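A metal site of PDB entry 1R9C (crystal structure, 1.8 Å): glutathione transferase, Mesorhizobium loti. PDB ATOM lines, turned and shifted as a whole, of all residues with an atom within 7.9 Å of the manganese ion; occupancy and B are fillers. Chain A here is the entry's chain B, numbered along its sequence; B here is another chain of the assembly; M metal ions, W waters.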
ATOM      1  N   TYR A  67     -29.039  13.214   0.529  1.00  0.00           N
ATOM      2  CA  TYR A  67     -28.323  14.384   1.024  1.00  0.00           C
ATOM      3  C   TYR A  67     -27.044  14.737   0.223  1.00  0.00           C
ATOM      4  O   TYR A  67     -26.274  15.604   0.623  1.00  0.00           O
ATOM      5  CB  TYR A  67     -28.039  14.221   2.533  1.00  0.00           C
ATOM      6  CG  TYR A  67     -29.299  14.270   3.395  1.00  0.00           C
ATOM      7  CD1 TYR A  67     -29.359  13.579   4.595  1.00  0.00           C
ATOM      8  CD2 TYR A  67     -30.404  15.033   3.016  1.00  0.00           C
ATOM      9  CE1 TYR A  67     -30.508  13.619   5.396  1.00  0.00           C
ATOM     10  CE2 TYR A  67     -31.561  15.093   3.813  1.00  0.00           C
ATOM     11  CZ  TYR A  67     -31.596  14.371   5.004  1.00  0.00           C
ATOM     12  OH  TYR A  67     -32.737  14.421   5.787  1.00  0.00           O
ATOM     13  N   HIS A  69     -25.398  16.936  -2.457  1.00  0.00           N
ATOM     14  CA  HIS A  69     -25.780  18.342  -2.715  1.00  0.00           C
ATOM     15  C   HIS A  69     -24.644  19.143  -3.308  1.00  0.00           C
ATOM     16  O   HIS A  69     -23.454  18.811  -3.150  1.00  0.00           O
ATOM     17  CB  HIS A  69     -26.386  19.054  -1.444  1.00  0.00           C
ATOM     18  CG  HIS A  69     -25.417  19.283  -0.298  1.00  0.00           C
ATOM     19  ND1 HIS A  69     -25.267  18.382   0.726  1.00  0.00           N
ATOM     20  CD2 HIS A  69     -24.656  20.367   0.032  1.00  0.00           C
ATOM     21  CE1 HIS A  69     -24.413  18.869   1.619  1.00  0.00           C
ATOM     22  NE2 HIS A  69     -24.021  20.070   1.223  1.00  0.00           N
ATOM     23  N   ILE A  70     -25.038  20.181  -4.033  1.00  0.00           N
ATOM     24  CA  ILE A  70     -24.097  21.177  -4.528  1.00  0.00           C
ATOM     25  C   ILE A  70     -24.374  22.464  -3.795  1.00  0.00           C
ATOM     26  O   ILE A  70     -25.526  22.892  -3.711  1.00  0.00           O
ATOM     27  CB  ILE A  70     -24.268  21.394  -6.038  1.00  0.00           C
ATOM     28  CG1 ILE A  70     -23.977  20.091  -6.849  1.00  0.00           C
ATOM     29  CG2 ILE A  70     -23.404  22.599  -6.514  1.00  0.00           C
ATOM     30  CD1 ILE A  70     -22.657  19.488  -6.591  1.00  0.00           C
ATOM     31  N   ALA A  71     -23.301  23.102  -3.320  1.00  0.00           N
ATOM     32  CA  ALA A  71     -23.442  24.307  -2.530  1.00  0.00           C
ATOM     33  C   ALA A  71     -22.699  25.486  -3.160  1.00  0.00           C
ATOM     34  O   ALA A  71     -21.550  25.353  -3.621  1.00  0.00           O
ATOM     35  CB  ALA A  71     -22.967  24.063  -1.127  1.00  0.00           C
ATOM     36  N   PHE A  72     -23.401  26.632  -3.165  1.00  0.00           N
ATOM     37  CA  PHE A  72     -22.871  27.868  -3.716  1.00  0.00           C
ATOM     38  C   PHE A  72     -22.608  28.841  -2.590  1.00  0.00           C
ATOM     39  O   PHE A  72     -23.321  28.854  -1.585  1.00  0.00           O
ATOM     40  CB  PHE A  72     -23.853  28.469  -4.730  1.00  0.00           C
ATOM     41  CG  PHE A  72     -23.963  27.661  -5.999  1.00  0.00           C
ATOM     42  CD1 PHE A  72     -25.018  26.769  -6.162  1.00  0.00           C
ATOM     43  CD2 PHE A  72     -23.003  27.764  -6.977  1.00  0.00           C
ATOM     44  CE1 PHE A  72     -25.126  25.993  -7.331  1.00  0.00           C
ATOM     45  CE2 PHE A  72     -23.087  27.014  -8.160  1.00  0.00           C
ATOM     46  CZ  PHE A  72     -24.146  26.114  -8.329  1.00  0.00           C
ATOM     47  N   SER A 106     -26.584  28.215   6.374  1.00  0.00           N
ATOM     48  CA  SER A 106     -26.974  27.601   5.079  1.00  0.00           C
ATOM     49  C   SER A 106     -28.480  27.646   4.813  1.00  0.00           C
ATOM     50  O   SER A 106     -29.281  27.598   5.739  1.00  0.00           O
ATOM     51  CB  SER A 106     -26.554  26.129   5.005  1.00  0.00           C
ATOM     52  OG  SER A 106     -25.155  25.963   5.037  1.00  0.00           O
ATOM     53  N   TYR A 108     -30.971  25.218   2.580  1.00  0.00           N
ATOM     54  CA  TYR A 108     -31.065  23.990   1.811  1.00  0.00           C
ATOM     55  C   TYR A 108     -32.420  23.933   1.134  1.00  0.00           C
ATOM     56  O   TYR A 108     -33.415  24.268   1.761  1.00  0.00           O
ATOM     57  CB  TYR A 108     -30.921  22.756   2.729  1.00  0.00           C
ATOM     58  CG  TYR A 108     -29.562  22.642   3.419  1.00  0.00           C
ATOM     59  CD1 TYR A 108     -29.399  23.127   4.708  1.00  0.00           C
ATOM     60  CD2 TYR A 108     -28.473  22.012   2.803  1.00  0.00           C
ATOM     61  CE1 TYR A 108     -28.195  23.019   5.365  1.00  0.00           C
ATOM     62  CE2 TYR A 108     -27.223  21.903   3.465  1.00  0.00           C
ATOM     63  CZ  TYR A 108     -27.119  22.430   4.756  1.00  0.00           C
ATOM     64  OH  TYR A 108     -25.938  22.372   5.504  1.00  0.00           O
ATOM     65  N   MET A 116     -30.793  18.305  -4.454  1.00  0.00           N
ATOM     66  CA  MET A 116     -30.590  19.205  -3.334  1.00  0.00           C
ATOM     67  C   MET A 116     -29.485  20.239  -3.628  1.00  0.00           C
ATOM     68  O   MET A 116     -28.385  19.898  -4.081  1.00  0.00           O
ATOM     69  CB  MET A 116     -30.281  18.454  -2.058  1.00  0.00           C
ATOM     70  CG  MET A 116     -30.154  19.408  -0.799  1.00  0.00           C
ATOM     71  SD  MET A 116     -29.583  18.467   0.651  1.00  0.00           S
ATOM     72  CE  MET A 116     -31.188  18.226   1.372  1.00  0.00           C
ATOM     73  N   PHE A 117     -29.808  21.503  -3.355  1.00  0.00           N
ATOM     74  CA  PHE A 117     -28.884  22.623  -3.467  1.00  0.00           C
ATOM     75  C   PHE A 117     -28.756  23.273  -2.123  1.00  0.00           C
ATOM     76  O   PHE A 117     -29.649  23.136  -1.287  1.00  0.00           O
ATOM     77  CB  PHE A 117     -29.429  23.643  -4.483  1.00  0.00           C
ATOM     78  CG  PHE A 117     -29.325  23.160  -5.897  1.00  0.00           C
ATOM     79  CD1 PHE A 117     -30.405  22.548  -6.510  1.00  0.00           C
ATOM     80  CD2 PHE A 117     -28.118  23.253  -6.591  1.00  0.00           C
ATOM     81  CE1 PHE A 117     -30.330  22.079  -7.833  1.00  0.00           C
ATOM     82  CE2 PHE A 117     -28.017  22.810  -7.911  1.00  0.00           C
ATOM     83  CZ  PHE A 117     -29.139  22.213  -8.536  1.00  0.00           C
ATOM     84  N   GLU A 118     -27.649  23.993  -1.924  1.00  0.00           N
ATOM     85  CA  GLU A 118     -27.354  24.673  -0.675  1.00  0.00           C
ATOM     86  C   GLU A 118     -26.759  26.046  -1.021  1.00  0.00           C
ATOM     87  O   GLU A 118     -25.998  26.183  -1.987  1.00  0.00           O
ATOM     88  CB  GLU A 118     -26.373  23.836   0.153  1.00  0.00           C
ATOM     89  CG  GLU A 118     -25.757  24.574   1.348  1.00  0.00           C
ATOM     90  CD  GLU A 118     -24.734  23.773   2.154  1.00  0.00           C
ATOM     91  OE1 GLU A 118     -24.321  22.627   1.809  1.00  0.00           O
ATOM     92  OE2 GLU A 118     -24.331  24.342   3.213  1.00  0.00           O
ATOM     93  N   LEU A 119     -27.165  27.076  -0.273  1.00  0.00           N
ATOM     94  CA  LEU A 119     -26.507  28.375  -0.326  1.00  0.00           C
ATOM     95  C   LEU A 119     -25.849  28.519   1.029  1.00  0.00           C
ATOM     96  O   LEU A 119     -26.495  28.362   2.057  1.00  0.00           O
ATOM     97  CB  LEU A 119     -27.496  29.530  -0.570  1.00  0.00           C
ATOM     98  CG  LEU A 119     -28.321  29.408  -1.864  1.00  0.00           C
ATOM     99  CD1 LEU A 119     -29.559  30.275  -1.811  1.00  0.00           C
ATOM    100  CD2 LEU A 119     -27.462  29.723  -3.134  1.00  0.00           C
ATOM    101  N   HIS A 120     -24.551  28.811   1.033  1.00  0.00           N
ATOM    102  CA  HIS A 120     -23.767  28.715   2.251  1.00  0.00           C
ATOM    103  C   HIS A 120     -22.954  30.007   2.412  1.00  0.00           C
ATOM    104  O   HIS A 120     -22.318  30.446   1.462  1.00  0.00           O
ATOM    105  CB  HIS A 120     -22.855  27.470   2.164  1.00  0.00           C
ATOM    106  CG  HIS A 120     -21.985  27.266   3.364  1.00  0.00           C
ATOM    107  ND1 HIS A 120     -22.478  27.278   4.656  1.00  0.00           N
ATOM    108  CD2 HIS A 120     -20.650  27.065   3.484  1.00  0.00           C
ATOM    109  CE1 HIS A 120     -21.486  27.072   5.510  1.00  0.00           C
ATOM    110  NE2 HIS A 120     -20.370  26.929   4.815  1.00  0.00           N
ATOM    111  N   ARG A 127     -14.706  26.757   8.624  1.00  0.00           N
ATOM    112  CA  ARG A 127     -15.222  25.450   9.026  1.00  0.00           C
ATOM    113  C   ARG A 127     -14.129  24.602   9.689  1.00  0.00           C
ATOM    114  O   ARG A 127     -14.384  23.926  10.692  1.00  0.00           O
ATOM    115  CB  ARG A 127     -15.859  24.737   7.828  1.00  0.00           C
ATOM    116  CG  ARG A 127     -16.397  23.354   8.115  1.00  0.00           C
ATOM    117  CD  ARG A 127     -17.875  23.168   7.816  1.00  0.00           C
ATOM    118  NE  ARG A 127     -18.412  22.111   8.669  1.00  0.00           N
ATOM    119  CZ  ARG A 127     -19.294  21.191   8.270  1.00  0.00           C
ATOM    120  NH1 ARG A 127     -19.756  21.202   7.028  1.00  0.00           N
ATOM    121  NH2 ARG A 127     -19.709  20.267   9.134  1.00  0.00           N
ATOM    122  N   SER B   6     -19.186  26.842  -3.332  1.00  0.00           N
ATOM    123  CA  SER B   6     -18.707  26.600  -1.970  1.00  0.00           C
ATOM    124  C   SER B   6     -18.125  25.196  -1.882  1.00  0.00           C
ATOM    125  O   SER B   6     -16.920  25.005  -1.618  1.00  0.00           O
ATOM    126  CB  SER B   6     -19.848  26.790  -0.963  1.00  0.00           C
ATOM    127  OG  SER B   6     -19.455  26.401   0.348  1.00  0.00           O
ATOM    128  N   HIS B   7     -18.971  24.188  -2.096  1.00  0.00           N
ATOM    129  CA  HIS B   7     -18.536  22.797  -2.001  1.00  0.00           C
ATOM    130  C   HIS B   7     -19.476  21.869  -2.766  1.00  0.00           C
ATOM    131  O   HIS B   7     -20.574  22.283  -3.166  1.00  0.00           O
ATOM    132  CB  HIS B   7     -18.410  22.352  -0.515  1.00  0.00           C
ATOM    133  CG  HIS B   7     -19.672  22.467   0.313  1.00  0.00           C
ATOM    134  ND1 HIS B   7     -20.018  23.616   0.987  1.00  0.00           N
ATOM    135  CD2 HIS B   7     -20.607  21.535   0.664  1.00  0.00           C
ATOM    136  CE1 HIS B   7     -21.131  23.409   1.685  1.00  0.00           C
ATOM    137  NE2 HIS B   7     -21.504  22.148   1.519  1.00  0.00           N
ATOM    138  N   MET B   8     -19.008  20.650  -3.050  1.00  0.00           N
ATOM    139  CA  MET B   8     -19.896  19.578  -3.458  1.00  0.00           C
ATOM    140  C   MET B   8     -19.794  18.441  -2.445  1.00  0.00           C
ATOM    141  O   MET B   8     -18.701  18.122  -1.955  1.00  0.00           O
ATOM    142  CB  MET B   8     -19.551  19.112  -4.889  1.00  0.00           C
ATOM    143  CG  MET B   8     -18.117  18.592  -4.997  1.00  0.00           C
ATOM    144  SD  MET B   8     -17.606  18.148  -6.692  1.00  0.00           S
ATOM    145  CE  MET B   8     -17.544  19.780  -7.451  1.00  0.00           C
ATOM    146  N   THR B   9     -20.943  17.849  -2.107  1.00  0.00           N
ATOM    147  CA  THR B   9     -20.980  16.818  -1.074  1.00  0.00           C
ATOM    148  C   THR B   9     -21.547  15.545  -1.637  1.00  0.00           C
ATOM    149  O   THR B   9     -22.642  15.552  -2.209  1.00  0.00           O
ATOM    150  CB  THR B   9     -21.826  17.311   0.126  1.00  0.00           C
ATOM    151  OG1 THR B   9     -21.085  18.296   0.835  1.00  0.00           O
ATOM    152  CG2 THR B   9     -22.005  16.194   1.150  1.00  0.00           C
ATOM    153  N   PHE B  46     -13.124  16.028   4.295  1.00  0.00           N
ATOM    154  CA  PHE B  46     -13.092  17.133   3.347  1.00  0.00           C
ATOM    155  C   PHE B  46     -11.808  17.001   2.510  1.00  0.00           C
ATOM    156  O   PHE B  46     -10.712  16.673   3.046  1.00  0.00           O
ATOM    157  CB  PHE B  46     -13.013  18.483   4.051  1.00  0.00           C
ATOM    158  CG  PHE B  46     -14.208  18.813   4.923  1.00  0.00           C
ATOM    159  CD1 PHE B  46     -14.074  19.773   5.919  1.00  0.00           C
ATOM    160  CD2 PHE B  46     -15.454  18.216   4.703  1.00  0.00           C
ATOM    161  CE1 PHE B  46     -15.161  20.130   6.720  1.00  0.00           C
ATOM    162  CE2 PHE B  46     -16.538  18.538   5.515  1.00  0.00           C
ATOM    163  CZ  PHE B  46     -16.403  19.518   6.517  1.00  0.00           C
ATOM    164  N   TRP B  53     -13.609  22.454  -2.930  1.00  0.00           N
ATOM    165  CA  TRP B  53     -13.930  21.716  -1.711  1.00  0.00           C
ATOM    166  C   TRP B  53     -14.915  20.605  -2.039  1.00  0.00           C
ATOM    167  O   TRP B  53     -16.024  20.877  -2.511  1.00  0.00           O
ATOM    168  CB  TRP B  53     -14.553  22.704  -0.747  1.00  0.00           C
ATOM    169  CG  TRP B  53     -14.970  22.238   0.618  1.00  0.00           C
ATOM    170  CD1 TRP B  53     -14.750  21.029   1.220  1.00  0.00           C
ATOM    171  CD2 TRP B  53     -15.682  23.040   1.566  1.00  0.00           C
ATOM    172  NE1 TRP B  53     -15.313  21.032   2.480  1.00  0.00           N
ATOM    173  CE2 TRP B  53     -15.869  22.253   2.727  1.00  0.00           C
ATOM    174  CE3 TRP B  53     -16.188  24.346   1.542  1.00  0.00           C
ATOM    175  CZ2 TRP B  53     -16.537  22.733   3.865  1.00  0.00           C
ATOM    176  CZ3 TRP B  53     -16.828  24.836   2.683  1.00  0.00           C
ATOM    177  CH2 TRP B  53     -17.001  24.031   3.824  1.00  0.00           C
ATOM    178  N   ALA B  55     -16.726  17.394  -0.086  1.00  0.00           N
ATOM    179  CA  ALA B  55     -16.990  16.740   1.198  1.00  0.00           C
ATOM    180  C   ALA B  55     -17.594  15.370   0.934  1.00  0.00           C
ATOM    181  O   ALA B  55     -18.466  15.237   0.082  1.00  0.00           O
ATOM    182  CB  ALA B  55     -17.960  17.579   2.050  1.00  0.00           C
ATOM    183  N   MET B  57     -19.396  12.002   3.075  1.00  0.00           N
ATOM    184  CA  MET B  57     -19.937  11.486   4.337  1.00  0.00           C
ATOM    185  C   MET B  57     -20.396  10.056   4.131  1.00  0.00           C
ATOM    186  O   MET B  57     -20.886   9.718   3.070  1.00  0.00           O
ATOM    187  CB  MET B  57     -21.092  12.353   4.857  1.00  0.00           C
ATOM    188  CG  MET B  57     -20.954  13.888   4.627  1.00  0.00           C
ATOM    189  SD  MET B  57     -22.496  14.814   5.049  1.00  0.00           S
ATOM    190  CE  MET B  57     -23.243  13.656   6.355  1.00  0.00           C
HETATM  191 MN    MN M   1     -23.099  21.337   2.551  1.00  0.00          MN
HETATM  192  O   HOH W   1     -22.721  22.776   4.414  1.00  0.00           O
HETATM  193  O   HOH W   2     -21.786  19.555   3.229  1.00  0.00           O
HETATM  194  O   HOH W   3     -24.535  20.437   4.370  1.00  0.00           O
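The side-chain hydroxyl (OH) of Tyr 108 sits at hydrogen-bond distance from the side-chain carboxylate (OE2) of Glu 118, 3.4 Å away.
The side-chain carboxylate (OE2) of Glu 118 sits at hydrogen-bond distance from the side-chain hydroxyl (OG) of Ser 106 (2.6 Å).
The backbone carbonyl oxygen of Ile 70 is in hydrogen-bond range of the backbone NH of Glu 118 (3.0 Å).
O of Glu 118 sits at hydrogen-bond distance from N of Phe 72, 2.9 Å away.
The backbone carbonyl oxygen of His 69 sits at hydrogen-bond distance from the backbone NH of Thr 9 of chain B, at 2.9 Å.
A ring nitrogen (ND1) of His 69 lies within hydrogen-bond range of the backbone carbonyl oxygen (O) of Tyr 67, at 3.0 Å.
N of Ala 71 sits at hydrogen-bond distance from O of His 7 of chain B, at 2.9 Å.
ND1 of His 7 of chain B is in hydrogen-bond range of OG of Ser 6 of chain B.
The manganese ion is bound by the side-chain carboxylate of Glu 118 (1.9 Å), a ring nitrogen (NE2) of His 69 (2.1 Å), a ring nitrogen (NE2) of His 7 of chain B (2.1 Å), water W2 (2.3 Å), water W1 (2.4 Å) and water W3 (2.5 Å).
The manganese ion has six donor atoms within binding distance.
Water W1 bridges the side-chain carboxylate (OE2) of Glu 118 and the side-chain hydroxyl (OH) of Tyr 108.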
